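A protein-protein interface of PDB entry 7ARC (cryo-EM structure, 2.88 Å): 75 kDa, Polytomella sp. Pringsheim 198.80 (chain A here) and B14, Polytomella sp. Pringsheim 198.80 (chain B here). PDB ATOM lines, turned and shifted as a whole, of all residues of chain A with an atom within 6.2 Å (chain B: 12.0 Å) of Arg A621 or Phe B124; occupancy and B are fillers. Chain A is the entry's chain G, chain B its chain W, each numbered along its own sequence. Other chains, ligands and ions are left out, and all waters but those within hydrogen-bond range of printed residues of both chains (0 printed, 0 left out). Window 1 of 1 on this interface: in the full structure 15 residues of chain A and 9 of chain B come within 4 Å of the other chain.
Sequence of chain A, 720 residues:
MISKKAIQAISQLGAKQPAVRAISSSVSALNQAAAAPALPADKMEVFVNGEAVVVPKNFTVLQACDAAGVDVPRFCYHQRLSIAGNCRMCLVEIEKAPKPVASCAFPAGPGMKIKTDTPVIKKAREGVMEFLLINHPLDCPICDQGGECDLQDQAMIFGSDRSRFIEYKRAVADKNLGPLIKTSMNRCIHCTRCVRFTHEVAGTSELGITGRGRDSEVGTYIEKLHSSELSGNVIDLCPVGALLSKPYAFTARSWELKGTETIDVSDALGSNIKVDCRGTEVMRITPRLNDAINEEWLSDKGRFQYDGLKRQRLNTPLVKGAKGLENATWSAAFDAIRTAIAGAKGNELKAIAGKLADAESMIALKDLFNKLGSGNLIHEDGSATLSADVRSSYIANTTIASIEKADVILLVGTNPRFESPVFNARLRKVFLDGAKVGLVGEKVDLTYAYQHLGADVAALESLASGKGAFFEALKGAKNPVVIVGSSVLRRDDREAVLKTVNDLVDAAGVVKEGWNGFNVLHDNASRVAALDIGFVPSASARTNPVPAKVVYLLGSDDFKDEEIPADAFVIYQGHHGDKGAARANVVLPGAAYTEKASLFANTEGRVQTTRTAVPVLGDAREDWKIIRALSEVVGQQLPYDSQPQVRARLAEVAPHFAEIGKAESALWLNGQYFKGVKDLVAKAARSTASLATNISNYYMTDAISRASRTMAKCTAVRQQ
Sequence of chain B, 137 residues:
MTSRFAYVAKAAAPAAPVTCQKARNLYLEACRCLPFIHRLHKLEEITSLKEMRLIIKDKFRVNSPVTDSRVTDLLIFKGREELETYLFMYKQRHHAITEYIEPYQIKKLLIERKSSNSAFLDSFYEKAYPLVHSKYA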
ATOM      1  N   TRP A 330     -15.722  -8.428   2.516  1.00  0.00           N
ATOM      2  CA  TRP A 330     -14.902  -7.518   1.723  1.00  0.00           C
ATOM      3  C   TRP A 330     -15.094  -6.074   2.167  1.00  0.00           C
ATOM      4  O   TRP A 330     -14.140  -5.288   2.177  1.00  0.00           O
ATOM      5  CB  TRP A 330     -15.230  -7.672   0.242  1.00  0.00           C
ATOM      6  CG  TRP A 330     -14.440  -8.741  -0.432  1.00  0.00           C
ATOM      7  CD1 TRP A 330     -14.920  -9.906  -0.941  1.00  0.00           C
ATOM      8  CD2 TRP A 330     -13.028  -8.753  -0.665  1.00  0.00           C
ATOM      9  NE1 TRP A 330     -13.900 -10.645  -1.482  1.00  0.00           N
ATOM     10  CE2 TRP A 330     -12.726  -9.958  -1.326  1.00  0.00           C
ATOM     11  CE3 TRP A 330     -11.991  -7.862  -0.384  1.00  0.00           C
ATOM     12  CZ2 TRP A 330     -11.434 -10.293  -1.709  1.00  0.00           C
ATOM     13  CZ3 TRP A 330     -10.710  -8.198  -0.766  1.00  0.00           C
ATOM     14  CH2 TRP A 330     -10.442  -9.401  -1.421  1.00  0.00           C
ATOM     15  N   PHE A 334     -12.100  -3.568   3.674  1.00  0.00           N
ATOM     16  CA  PHE A 334     -11.840  -2.288   3.025  1.00  0.00           C
ATOM     17  C   PHE A 334     -12.025  -1.127   3.991  1.00  0.00           C
ATOM     18  O   PHE A 334     -11.286  -0.140   3.930  1.00  0.00           O
ATOM     19  CB  PHE A 334     -12.736  -2.128   1.803  1.00  0.00           C
ATOM     20  CG  PHE A 334     -12.310  -2.963   0.636  1.00  0.00           C
ATOM     21  CD1 PHE A 334     -11.030  -3.476   0.572  1.00  0.00           C
ATOM     22  CD2 PHE A 334     -13.186  -3.232  -0.396  1.00  0.00           C
ATOM     23  CE1 PHE A 334     -10.634  -4.243  -0.494  1.00  0.00           C
ATOM     24  CE2 PHE A 334     -12.792  -3.998  -1.465  1.00  0.00           C
ATOM     25  CZ  PHE A 334     -11.515  -4.504  -1.514  1.00  0.00           C
ATOM     26  N   GLN A 573      -1.985  -9.023   0.469  1.00  0.00           N
ATOM     27  CA  GLN A 573      -2.819  -9.472  -0.635  1.00  0.00           C
ATOM     28  C   GLN A 573      -2.121 -10.640  -1.314  1.00  0.00           C
ATOM     29  O   GLN A 573      -1.000 -10.493  -1.807  1.00  0.00           O
ATOM     30  CB  GLN A 573      -3.061  -8.340  -1.627  1.00  0.00           C
ATOM     31  CG  GLN A 573      -4.053  -8.675  -2.710  1.00  0.00           C
ATOM     32  CD  GLN A 573      -4.251  -7.530  -3.670  1.00  0.00           C
ATOM     33  OE1 GLN A 573      -3.826  -6.407  -3.410  1.00  0.00           O
ATOM     34  NE2 GLN A 573      -4.896  -7.806  -4.789  1.00  0.00           N
ATOM     35  N   PRO A 589      -7.778 -12.078   0.005  1.00  0.00           N
ATOM     36  CA  PRO A 589      -7.528 -13.230  -0.868  1.00  0.00           C
ATOM     37  C   PRO A 589      -7.459 -12.820  -2.330  1.00  0.00           C
ATOM     38  O   PRO A 589      -8.225 -11.975  -2.795  1.00  0.00           O
ATOM     39  CB  PRO A 589      -8.728 -14.144  -0.601  1.00  0.00           C
ATOM     40  CG  PRO A 589      -9.785 -13.237  -0.101  1.00  0.00           C
ATOM     41  CD  PRO A 589      -9.094 -12.151   0.656  1.00  0.00           C
ATOM     42  N   GLY A 590      -6.536 -13.445  -3.059  1.00  0.00           N
ATOM     43  CA  GLY A 590      -6.380 -13.183  -4.469  1.00  0.00           C
ATOM     44  C   GLY A 590      -6.249 -14.479  -5.244  1.00  0.00           C
ATOM     45  O   GLY A 590      -5.995 -15.542  -4.683  1.00  0.00           O
ATOM     46  N   ALA A 591      -6.460 -14.375  -6.550  1.00  0.00           N
ATOM     47  CA  ALA A 591      -6.340 -15.529  -7.424  1.00  0.00           C
ATOM     48  C   ALA A 591      -4.872 -15.847  -7.694  1.00  0.00           C
ATOM     49  O   ALA A 591      -3.988 -14.998  -7.550  1.00  0.00           O
ATOM     50  CB  ALA A 591      -7.073 -15.284  -8.742  1.00  0.00           C
ATOM     51  N   VAL A 616     -11.781 -19.161  -9.466  1.00  0.00           N
ATOM     52  CA  VAL A 616     -11.252 -18.641  -8.213  1.00  0.00           C
ATOM     53  C   VAL A 616     -11.951 -19.321  -7.043  1.00  0.00           C
ATOM     54  O   VAL A 616     -13.131 -19.686  -7.113  1.00  0.00           O
ATOM     55  CB  VAL A 616     -11.398 -17.110  -8.137  1.00  0.00           C
ATOM     56  CG1 VAL A 616     -10.607 -16.451  -9.246  1.00  0.00           C
ATOM     57  CG2 VAL A 616     -12.854 -16.715  -8.221  1.00  0.00           C
ATOM     58  N   LEU A 617     -11.209 -19.501  -5.958  1.00  0.00           N
ATOM     59  CA  LEU A 617     -11.657 -20.262  -4.802  1.00  0.00           C
ATOM     60  C   LEU A 617     -12.260 -19.347  -3.749  1.00  0.00           C
ATOM     61  O   LEU A 617     -11.673 -18.317  -3.403  1.00  0.00           O
ATOM     62  CB  LEU A 617     -10.487 -21.030  -4.191  1.00  0.00           C
ATOM     63  CG  LEU A 617     -10.835 -21.922  -3.004  1.00  0.00           C
ATOM     64  CD1 LEU A 617     -11.800 -23.025  -3.409  1.00  0.00           C
ATOM     65  CD2 LEU A 617      -9.577 -22.482  -2.391  1.00  0.00           C
ATOM     66  N   GLY A 618     -13.421 -19.742  -3.231  1.00  0.00           N
ATOM     67  CA  GLY A 618     -14.016 -19.035  -2.112  1.00  0.00           C
ATOM     68  C   GLY A 618     -14.343 -17.602  -2.467  1.00  0.00           C
ATOM     69  O   GLY A 618     -14.752 -17.287  -3.588  1.00  0.00           O
ATOM     70  N   ASP A 619     -14.173 -16.716  -1.493  1.00  0.00           N
ATOM     71  CA  ASP A 619     -14.442 -15.294  -1.682  1.00  0.00           C
ATOM     72  C   ASP A 619     -13.162 -14.551  -2.061  1.00  0.00           C
ATOM     73  O   ASP A 619     -12.787 -13.555  -1.449  1.00  0.00           O
ATOM     74  CB  ASP A 619     -15.071 -14.724  -0.416  1.00  0.00           C
ATOM     75  CG  ASP A 619     -15.584 -13.310  -0.595  1.00  0.00           C
ATOM     76  OD1 ASP A 619     -15.432 -12.748  -1.698  1.00  0.00           O
ATOM     77  OD2 ASP A 619     -16.151 -12.760   0.371  1.00  0.00           O
ATOM     78  N   ALA A 620     -12.473 -15.049  -3.084  1.00  0.00           N
ATOM     79  CA  ALA A 620     -11.278 -14.419  -3.623  1.00  0.00           C
ATOM     80  C   ALA A 620     -11.585 -13.745  -4.953  1.00  0.00           C
ATOM     81  O   ALA A 620     -12.536 -14.103  -5.652  1.00  0.00           O
ATOM     82  CB  ALA A 620     -10.155 -15.444  -3.805  1.00  0.00           C
ATOM     83  N   ARG A 621     -10.758 -12.760  -5.303  1.00  0.00           N
ATOM     84  CA  ARG A 621     -10.992 -11.942  -6.482  1.00  0.00           C
ATOM     85  C   ARG A 621      -9.677 -11.736  -7.221  1.00  0.00           C
ATOM     86  O   ARG A 621      -8.597 -11.982  -6.683  1.00  0.00           O
ATOM     87  CB  ARG A 621     -11.584 -10.578  -6.102  1.00  0.00           C
ATOM     88  CG  ARG A 621     -12.834 -10.643  -5.239  1.00  0.00           C
ATOM     89  CD  ARG A 621     -14.095 -10.818  -6.051  1.00  0.00           C
ATOM     90  NE  ARG A 621     -15.280 -10.646  -5.221  1.00  0.00           N
ATOM     91  CZ  ARG A 621     -15.941 -11.640  -4.647  1.00  0.00           C
ATOM     92  NH1 ARG A 621     -15.561 -12.897  -4.794  1.00  0.00           N
ATOM     93  NH2 ARG A 621     -17.008 -11.366  -3.904  1.00  0.00           N
ATOM     94  N   GLU A 622      -9.779 -11.290  -8.472  1.00  0.00           N
ATOM     95  CA  GLU A 622      -8.591 -10.885  -9.215  1.00  0.00           C
ATOM     96  C   GLU A 622      -7.930  -9.681  -8.556  1.00  0.00           C
ATOM     97  O   GLU A 622      -8.603  -8.766  -8.078  1.00  0.00           O
ATOM     98  CB  GLU A 622      -8.943 -10.574 -10.667  1.00  0.00           C
ATOM     99  CG  GLU A 622      -9.382 -11.792 -11.458  1.00  0.00           C
ATOM    100  CD  GLU A 622      -9.739 -11.458 -12.891  1.00  0.00           C
ATOM    101  OE1 GLU A 622      -9.762 -10.259 -13.235  1.00  0.00           O
ATOM    102  OE2 GLU A 622      -9.991 -12.399 -13.675  1.00  0.00           O
ATOM    103  N   ASP A 623      -6.595  -9.684  -8.547  1.00  0.00           N
ATOM    104  CA  ASP A 623      -5.846  -8.747  -7.715  1.00  0.00           C
ATOM    105  C   ASP A 623      -6.024  -7.298  -8.157  1.00  0.00           C
ATOM    106  O   ASP A 623      -6.193  -6.405  -7.317  1.00  0.00           O
ATOM    107  CB  ASP A 623      -4.369  -9.133  -7.717  1.00  0.00           C
ATOM    108  CG  ASP A 623      -4.144 -10.567  -7.278  1.00  0.00           C
ATOM    109  OD1 ASP A 623      -4.484 -11.486  -8.050  1.00  0.00           O
ATOM    110  OD2 ASP A 623      -3.624 -10.774  -6.162  1.00  0.00           O
ATOM    111  N   LYS A 625      -8.574  -6.062  -9.658  1.00  0.00           N
ATOM    112  CA  LYS A 625      -9.919  -5.690  -9.231  1.00  0.00           C
ATOM    113  C   LYS A 625      -9.955  -5.366  -7.745  1.00  0.00           C
ATOM    114  O   LYS A 625     -10.655  -4.440  -7.323  1.00  0.00           O
ATOM    115  CB  LYS A 625     -10.908  -6.807  -9.554  1.00  0.00           C
ATOM    116  CG  LYS A 625     -11.056  -7.103 -11.028  1.00  0.00           C
ATOM    117  CD  LYS A 625     -12.437  -7.648 -11.332  1.00  0.00           C
ATOM    118  CE  LYS A 625     -12.457  -8.397 -12.650  1.00  0.00           C
ATOM    119  NZ  LYS A 625     -13.676  -8.086 -13.445  1.00  0.00           N
ATOM    120  N   ILE A 626      -9.192  -6.105  -6.937  1.00  0.00           N
ATOM    121  CA  ILE A 626      -9.127  -5.818  -5.507  1.00  0.00           C
ATOM    122  C   ILE A 626      -8.557  -4.428  -5.278  1.00  0.00           C
ATOM    123  O   ILE A 626      -9.083  -3.640  -4.483  1.00  0.00           O
ATOM    124  CB  ILE A 626      -8.292  -6.885  -4.779  1.00  0.00           C
ATOM    125  CG1 ILE A 626      -8.946  -8.258  -4.896  1.00  0.00           C
ATOM    126  CG2 ILE A 626      -8.094  -6.505  -3.323  1.00  0.00           C
ATOM    127  CD1 ILE A 626      -8.000  -9.386  -4.620  1.00  0.00           C
ATOM    128  N   ILE A 627      -7.471  -4.103  -5.980  1.00  0.00           N
ATOM    129  CA  ILE A 627      -6.833  -2.809  -5.774  1.00  0.00           C
ATOM    130  C   ILE A 627      -7.734  -1.682  -6.262  1.00  0.00           C
ATOM    131  O   ILE A 627      -7.812  -0.624  -5.632  1.00  0.00           O
ATOM    132  CB  ILE A 627      -5.454  -2.769  -6.453  1.00  0.00           C
ATOM    133  CG1 ILE A 627      -4.510  -3.775  -5.797  1.00  0.00           C
ATOM    134  CG2 ILE A 627      -4.862  -1.381  -6.361  1.00  0.00           C
ATOM    135  CD1 ILE A 627      -3.541  -4.413  -6.750  1.00  0.00           C
ATOM    136  N   ALA A 629     -11.087  -1.721  -6.404  1.00  0.00           N
ATOM    137  CA  ALA A 629     -12.167  -1.586  -5.433  1.00  0.00           C
ATOM    138  C   ALA A 629     -11.693  -0.860  -4.182  1.00  0.00           C
ATOM    139  O   ALA A 629     -12.396   0.009  -3.652  1.00  0.00           O
ATOM    140  CB  ALA A 629     -12.724  -2.963  -5.078  1.00  0.00           C
ATOM    141  N   LEU A 630     -10.495  -1.195  -3.701  1.00  0.00           N
ATOM    142  CA  LEU A 630      -9.938  -0.486  -2.557  1.00  0.00           C
ATOM    143  C   LEU A 630      -9.711   0.985  -2.879  1.00  0.00           C
ATOM    144  O   LEU A 630      -9.890   1.851  -2.018  1.00  0.00           O
ATOM    145  CB  LEU A 630      -8.633  -1.150  -2.123  1.00  0.00           C
ATOM    146  CG  LEU A 630      -7.902  -0.500  -0.953  1.00  0.00           C
ATOM    147  CD1 LEU A 630      -8.799  -0.445   0.266  1.00  0.00           C
ATOM    148  CD2 LEU A 630      -6.628  -1.258  -0.655  1.00  0.00           C
ATOM    149  N   SER B 115     -27.711   3.049  -4.578  1.00  0.00           N
ATOM    150  CA  SER B 115     -26.421   2.638  -4.046  1.00  0.00           C
ATOM    151  C   SER B 115     -25.380   3.729  -4.262  1.00  0.00           C
ATOM    152  O   SER B 115     -25.197   4.219  -5.380  1.00  0.00           O
ATOM    153  CB  SER B 115     -25.970   1.336  -4.703  1.00  0.00           C
ATOM    154  OG  SER B 115     -26.810   0.261  -4.324  1.00  0.00           O
ATOM    155  N   ASN B 117     -22.193   3.184  -3.804  1.00  0.00           N
ATOM    156  CA  ASN B 117     -21.115   2.493  -4.493  1.00  0.00           C
ATOM    157  C   ASN B 117     -21.369   2.490  -5.994  1.00  0.00           C
ATOM    158  O   ASN B 117     -22.508   2.350  -6.447  1.00  0.00           O
ATOM    159  CB  ASN B 117     -21.006   1.057  -3.986  1.00  0.00           C
ATOM    160  CG  ASN B 117     -20.532   0.982  -2.554  1.00  0.00           C
ATOM    161  OD1 ASN B 117     -19.690   1.769  -2.124  1.00  0.00           O
ATOM    162  ND2 ASN B 117     -21.073   0.032  -1.804  1.00  0.00           N
ATOM    163  N   SER B 118     -20.299   2.645  -6.770  1.00  0.00           N
ATOM    164  CA  SER B 118     -20.424   2.622  -8.218  1.00  0.00           C
ATOM    165  C   SER B 118     -20.802   1.219  -8.690  1.00  0.00           C
ATOM    166  O   SER B 118     -20.913   0.274  -7.906  1.00  0.00           O
ATOM    167  CB  SER B 118     -19.128   3.090  -8.874  1.00  0.00           C
ATOM    168  OG  SER B 118     -18.071   2.182  -8.628  1.00  0.00           O
ATOM    169  N   ALA B 119     -21.010   1.090 -10.001  1.00  0.00           N
ATOM    170  CA  ALA B 119     -21.413  -0.196 -10.561  1.00  0.00           C
ATOM    171  C   ALA B 119     -20.337  -1.255 -10.360  1.00  0.00           C
ATOM    172  O   ALA B 119     -20.649  -2.425 -10.116  1.00  0.00           O
ATOM    173  CB  ALA B 119     -21.741  -0.040 -12.045  1.00  0.00           C
ATOM    174  N   PHE B 120     -19.065  -0.866 -10.469  1.00  0.00           N
ATOM    175  CA  PHE B 120     -17.978  -1.824 -10.294  1.00  0.00           C
ATOM    176  C   PHE B 120     -17.943  -2.370  -8.871  1.00  0.00           C
ATOM    177  O   PHE B 120     -17.785  -3.577  -8.661  1.00  0.00           O
ATOM    178  CB  PHE B 120     -16.640  -1.173 -10.648  1.00  0.00           C
ATOM    179  CG  PHE B 120     -15.469  -2.112 -10.571  1.00  0.00           C
ATOM    180  CD1 PHE B 120     -14.816  -2.336  -9.370  1.00  0.00           C
ATOM    181  CD2 PHE B 120     -15.017  -2.764 -11.703  1.00  0.00           C
ATOM    182  CE1 PHE B 120     -13.750  -3.201  -9.299  1.00  0.00           C
ATOM    183  CE2 PHE B 120     -13.945  -3.626 -11.638  1.00  0.00           C
ATOM    184  CZ  PHE B 120     -13.311  -3.843 -10.434  1.00  0.00           C
ATOM    185  N   LEU B 121     -18.065  -1.487  -7.877  1.00  0.00           N
ATOM    186  CA  LEU B 121     -17.970  -1.916  -6.485  1.00  0.00           C
ATOM    187  C   LEU B 121     -19.073  -2.904  -6.121  1.00  0.00           C
ATOM    188  O   LEU B 121     -18.826  -3.882  -5.405  1.00  0.00           O
ATOM    189  CB  LEU B 121     -18.003  -0.703  -5.558  1.00  0.00           C
ATOM    190  CG  LEU B 121     -17.349  -0.932  -4.197  1.00  0.00           C
ATOM    191  CD1 LEU B 121     -16.027  -1.647  -4.367  1.00  0.00           C
ATOM    192  CD2 LEU B 121     -17.145   0.381  -3.473  1.00  0.00           C
ATOM    193  N   ASP B 122     -20.296  -2.660  -6.589  1.00  0.00           N
ATOM    194  CA  ASP B 122     -21.408  -3.540  -6.248  1.00  0.00           C
ATOM    195  C   ASP B 122     -21.193  -4.939  -6.812  1.00  0.00           C
ATOM    196  O   ASP B 122     -21.393  -5.942  -6.116  1.00  0.00           O
ATOM    197  CB  ASP B 122     -22.718  -2.942  -6.759  1.00  0.00           C
ATOM    198  CG  ASP B 122     -23.190  -1.777  -5.913  1.00  0.00           C
ATOM    199  OD1 ASP B 122     -22.877  -1.754  -4.705  1.00  0.00           O
ATOM    200  OD2 ASP B 122     -23.872  -0.883  -6.456  1.00  0.00           O
ATOM    201  N   SER B 123     -20.780  -5.027  -8.076  1.00  0.00           N
ATOM    202  CA  SER B 123     -20.526  -6.330  -8.680  1.00  0.00           C
ATOM    203  C   SER B 123     -19.329  -7.011  -8.030  1.00  0.00           C
ATOM    204  O   SER B 123     -19.306  -8.239  -7.894  1.00  0.00           O
ATOM    205  CB  SER B 123     -20.318  -6.182 -10.186  1.00  0.00           C
ATOM    206  OG  SER B 123     -19.201  -5.362 -10.468  1.00  0.00           O
ATOM    207  N   PHE B 124     -18.315  -6.232  -7.641  1.00  0.00           N
ATOM    208  CA  PHE B 124     -17.171  -6.798  -6.931  1.00  0.00           C
ATOM    209  C   PHE B 124     -17.595  -7.412  -5.603  1.00  0.00           C
ATOM    210  O   PHE B 124     -17.147  -8.507  -5.246  1.00  0.00           O
ATOM    211  CB  PHE B 124     -16.117  -5.713  -6.709  1.00  0.00           C
ATOM    212  CG  PHE B 124     -14.937  -6.162  -5.896  1.00  0.00           C
ATOM    213  CD1 PHE B 124     -13.863  -6.785  -6.501  1.00  0.00           C
ATOM    214  CD2 PHE B 124     -14.895  -5.946  -4.530  1.00  0.00           C
ATOM    215  CE1 PHE B 124     -12.776  -7.190  -5.758  1.00  0.00           C
ATOM    216  CE2 PHE B 124     -13.811  -6.353  -3.785  1.00  0.00           C
ATOM    217  CZ  PHE B 124     -12.751  -6.974  -4.399  1.00  0.00           C
ATOM    218  N   TYR B 125     -18.455  -6.719  -4.857  1.00  0.00           N
ATOM    219  CA  TYR B 125     -18.965  -7.275  -3.608  1.00  0.00           C
ATOM    220  C   TYR B 125     -19.836  -8.498  -3.854  1.00  0.00           C
ATOM    221  O   TYR B 125     -19.841  -9.434  -3.048  1.00  0.00           O
ATOM    222  CB  TYR B 125     -19.749  -6.221  -2.831  1.00  0.00           C
ATOM    223  CG  TYR B 125     -18.900  -5.158  -2.183  1.00  0.00           C
ATOM    224  CD1 TYR B 125     -17.574  -5.401  -1.867  1.00  0.00           C
ATOM    225  CD2 TYR B 125     -19.430  -3.917  -1.870  1.00  0.00           C
ATOM    226  CE1 TYR B 125     -16.797  -4.434  -1.267  1.00  0.00           C
ATOM    227  CE2 TYR B 125     -18.662  -2.945  -1.271  1.00  0.00           C
ATOM    228  CZ  TYR B 125     -17.345  -3.209  -0.971  1.00  0.00           C
ATOM    229  OH  TYR B 125     -16.575  -2.242  -0.374  1.00  0.00           O
ATOM    230  N   GLU B 126     -20.587  -8.506  -4.956  1.00  0.00           N
ATOM    231  CA  GLU B 126     -21.542  -9.584  -5.191  1.00  0.00           C
ATOM    232  C   GLU B 126     -20.844 -10.892  -5.549  1.00  0.00           C
ATOM    233  O   GLU B 126     -20.955 -11.886  -4.824  1.00  0.00           O
ATOM    234  CB  GLU B 126     -22.527  -9.169  -6.284  1.00  0.00           C
ATOM    235  CG  GLU B 126     -23.409 -10.287  -6.804  1.00  0.00           C
ATOM    236  CD  GLU B 126     -24.014  -9.964  -8.157  1.00  0.00           C
ATOM    237  OE1 GLU B 126     -25.251  -9.811  -8.235  1.00  0.00           O
ATOM    238  OE2 GLU B 126     -23.254  -9.860  -9.141  1.00  0.00           O
ATOM    239  N   LYS B 127     -20.109 -10.917  -6.659  1.00  0.00           N
ATOM    240  CA  LYS B 127     -19.524 -12.165  -7.127  1.00  0.00           C
ATOM    241  C   LYS B 127     -18.226 -11.897  -7.873  1.00  0.00           C
ATOM    242  O   LYS B 127     -17.968 -10.786  -8.339  1.00  0.00           O
ATOM    243  CB  LYS B 127     -20.498 -12.948  -8.011  1.00  0.00           C
ATOM    244  CG  LYS B 127     -20.864 -12.262  -9.303  1.00  0.00           C
ATOM    245  CD  LYS B 127     -21.803 -13.135 -10.102  1.00  0.00           C
ATOM    246  CE  LYS B 127     -23.178 -13.160  -9.492  1.00  0.00           C
ATOM    247  NZ  LYS B 127     -24.138 -13.909 -10.344  1.00  0.00           N
ATOM    248  N   ALA B 128     -17.404 -12.944  -7.966  1.00  0.00           N
ATOM    249  CA  ALA B 128     -16.117 -12.831  -8.644  1.00  0.00           C
ATOM    250  C   ALA B 128     -16.280 -12.700 -10.153  1.00  0.00           C
ATOM    251  O   ALA B 128     -15.571 -11.913 -10.789  1.00  0.00           O
ATOM    252  CB  ALA B 128     -15.243 -14.036  -8.307  1.00  0.00           C
ATOM    253  N   TYR B 129     -17.194 -13.463 -10.748  1.00  0.00           N
ATOM    254  CA  TYR B 129     -17.392 -13.414 -12.194  1.00  0.00           C
ATOM    255  C   TYR B 129     -18.696 -12.702 -12.515  1.00  0.00           C
ATOM    256  O   TYR B 129     -19.774 -13.300 -12.396  1.00  0.00           O
ATOM    257  CB  TYR B 129     -17.399 -14.825 -12.789  1.00  0.00           C
ATOM    258  CG  TYR B 129     -16.116 -15.592 -12.591  1.00  0.00           C
ATOM    259  CD1 TYR B 129     -15.014 -15.347 -13.394  1.00  0.00           C
ATOM    260  CD2 TYR B 129     -16.010 -16.567 -11.612  1.00  0.00           C
ATOM    261  CE1 TYR B 129     -13.843 -16.041 -13.224  1.00  0.00           C
ATOM    262  CE2 TYR B 129     -14.839 -17.270 -11.435  1.00  0.00           C
ATOM    263  CZ  TYR B 129     -13.759 -17.001 -12.247  1.00  0.00           C
ATOM    264  OH  TYR B 129     -12.583 -17.693 -12.082  1.00  0.00           O
ATOM    265  N   PRO B 130     -18.654 -11.438 -12.943  1.00  0.00           N
ATOM    266  CA  PRO B 130     -19.905 -10.704 -13.188  1.00  0.00           C
ATOM    267  C   PRO B 130     -20.757 -11.297 -14.294  1.00  0.00           C
ATOM    268  O   PRO B 130     -21.974 -11.077 -14.303  1.00  0.00           O
ATOM    269  CB  PRO B 130     -19.417  -9.294 -13.549  1.00  0.00           C
ATOM    270  CG  PRO B 130     -18.025  -9.491 -14.038  1.00  0.00           C
ATOM    271  CD  PRO B 130     -17.466 -10.621 -13.232  1.00  0.00           C
ATOM    272  N   LEU B 131     -20.158 -12.028 -15.237  1.00  0.00           N
ATOM    273  CA  LEU B 131     -20.913 -12.530 -16.380  1.00  0.00           C
ATOM    274  C   LEU B 131     -21.931 -13.588 -15.975  1.00  0.00           C
ATOM    275  O   LEU B 131     -22.955 -13.745 -16.649  1.00  0.00           O
ATOM    276  CB  LEU B 131     -19.955 -13.078 -17.434  1.00  0.00           C
ATOM    277  CG  LEU B 131     -19.194 -12.000 -18.207  1.00  0.00           C
ATOM    278  CD1 LEU B 131     -18.435 -12.608 -19.366  1.00  0.00           C
ATOM    279  CD2 LEU B 131     -20.141 -10.917 -18.700  1.00  0.00           C
ATOM    280  N   VAL B 132     -21.665 -14.333 -14.901  1.00  0.00           N
ATOM    281  CA  VAL B 132     -22.630 -15.307 -14.406  1.00  0.00           C
ATOM    282  C   VAL B 132     -23.856 -14.587 -13.863  1.00  0.00           C
ATOM    283  O   VAL B 132     -23.745 -13.583 -13.147  1.00  0.00           O
ATOM    284  CB  VAL B 132     -21.991 -16.207 -13.336  1.00  0.00           C
ATOM    285  CG1 VAL B 132     -22.879 -17.408 -13.060  1.00  0.00           C
ATOM    286  CG2 VAL B 132     -20.609 -16.654 -13.774  1.00  0.00           C
ATOM    287  N   SER B 134     -27.410 -13.843 -11.744  1.00  0.00           N
ATOM    288  CA  SER B 134     -27.887 -13.971 -10.374  1.00  0.00           C
ATOM    289  C   SER B 134     -29.386 -14.228 -10.368  1.00  0.00           C
ATOM    290  O   SER B 134     -30.134 -13.593 -11.118  1.00  0.00           O
ATOM    291  CB  SER B 134     -27.583 -12.714  -9.558  1.00  0.00           C
ATOM    292  OG  SER B 134     -26.191 -12.513  -9.425  1.00  0.00           O
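Of the printed residues of chain B, Arg A621 touches Phe B124, Tyr B125, Lys B127 and Ala B128.
Of the printed residues of chain A, Phe B124 touches Phe A334 (3.5 Å), Arg A621 (2.8 Å), Lys A625 (3.8 Å), Ile A626 (3.9 Å) and Ala A629 (3.7 Å).
Of chain B, only Ala B128 and Tyr B129 come within 4 Å of Val A616.
Gly A618 touches none of the printed residues of chain B.
Ala A620 touches just one residue of chain B: Ala B128 (3.8 Å).
No residue of chain B comes within 4 Å of Glu A622.
Ile A626 touches one residue of chain B.
Printed residues of chain B within 4 Å of Ala A629: Leu B121 and Phe B124.
Of the printed residues of chain A, Leu B121 touches Ala A629 (3.6 Å).
Printed residues of chain A within 4 Å of Phe B120: Lys A625 (3.9 Å).
Printed residues of chain A within 4 Å of Lys B127: Arg A621.
Of the printed residues of chain A, Tyr B125 touches Trp A330 (3.9 Å), Phe A334 (3.5 Å) and Arg A621 (3.5 Å).
Gln A573 touches none of the printed residues of chain B.
Ser B134 touches none of the printed residues of chain A.
The nearest printed residue of chain A that does not touch Phe B124 is Trp A330 (4.01 Å).
Among the printed residues, merely in contact across the chains: Trp A330 with Tyr B125 (3.9 Å), Phe A334 with Phe B124 (3.5 Å), Phe A334 with Tyr B125 (3.5 Å), Val A616 with Ala B128 (3.6 Å), Ala A620 with Ala B128 (3.8 Å), Arg A621 with Tyr B125 (3.5 Å), Arg A621 with Lys B127 (3.96 Å), Arg A621 with Ala B128 (3.7 Å), Lys A625 with Phe B120 (3.9 Å), Lys A625 with Phe B124 (3.8 Å), Ile A626 with Phe B124 (3.9 Å), Ala A629 with Leu B121 (3.6 Å) and Ala A629 with Phe B124 (3.7 Å).
O of Phe B124 lies within hydrogen-bond range of NE of Arg A621, 2.8 Å away.
The side-chain hydroxyl (OH) of Tyr B129 is in hydrogen-bond range of the backbone NH (N) of Val A616 (3.1 Å).
The side-chain hydroxyl of Ser B123 sits at hydrogen-bond distance from the backbone carbonyl oxygen of Phe B120 (2.9 Å).
NZ of Lys B127 sits at hydrogen-bond distance from O of Val B132, 2.8 Å away.
OG of Ser B134 is in hydrogen-bond range of NZ of Lys B127 (2.6 Å).
The side-chain carboxylate of Asp A619 is in hydrogen-bond range of the indole nitrogen of Trp A330, 2.6 Å away.
O of Arg A621 is in hydrogen-bond range of N of Ala A591, at 3.2 Å.
OD1 of Asp A619 lies within salt-bridge range of NH2 of Arg A621 (3.0 Å).
Among the printed residues, no Asp or Glu carboxylate lies within 4 Å of a Lys or Arg side-chain nitrogen of the other chain.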
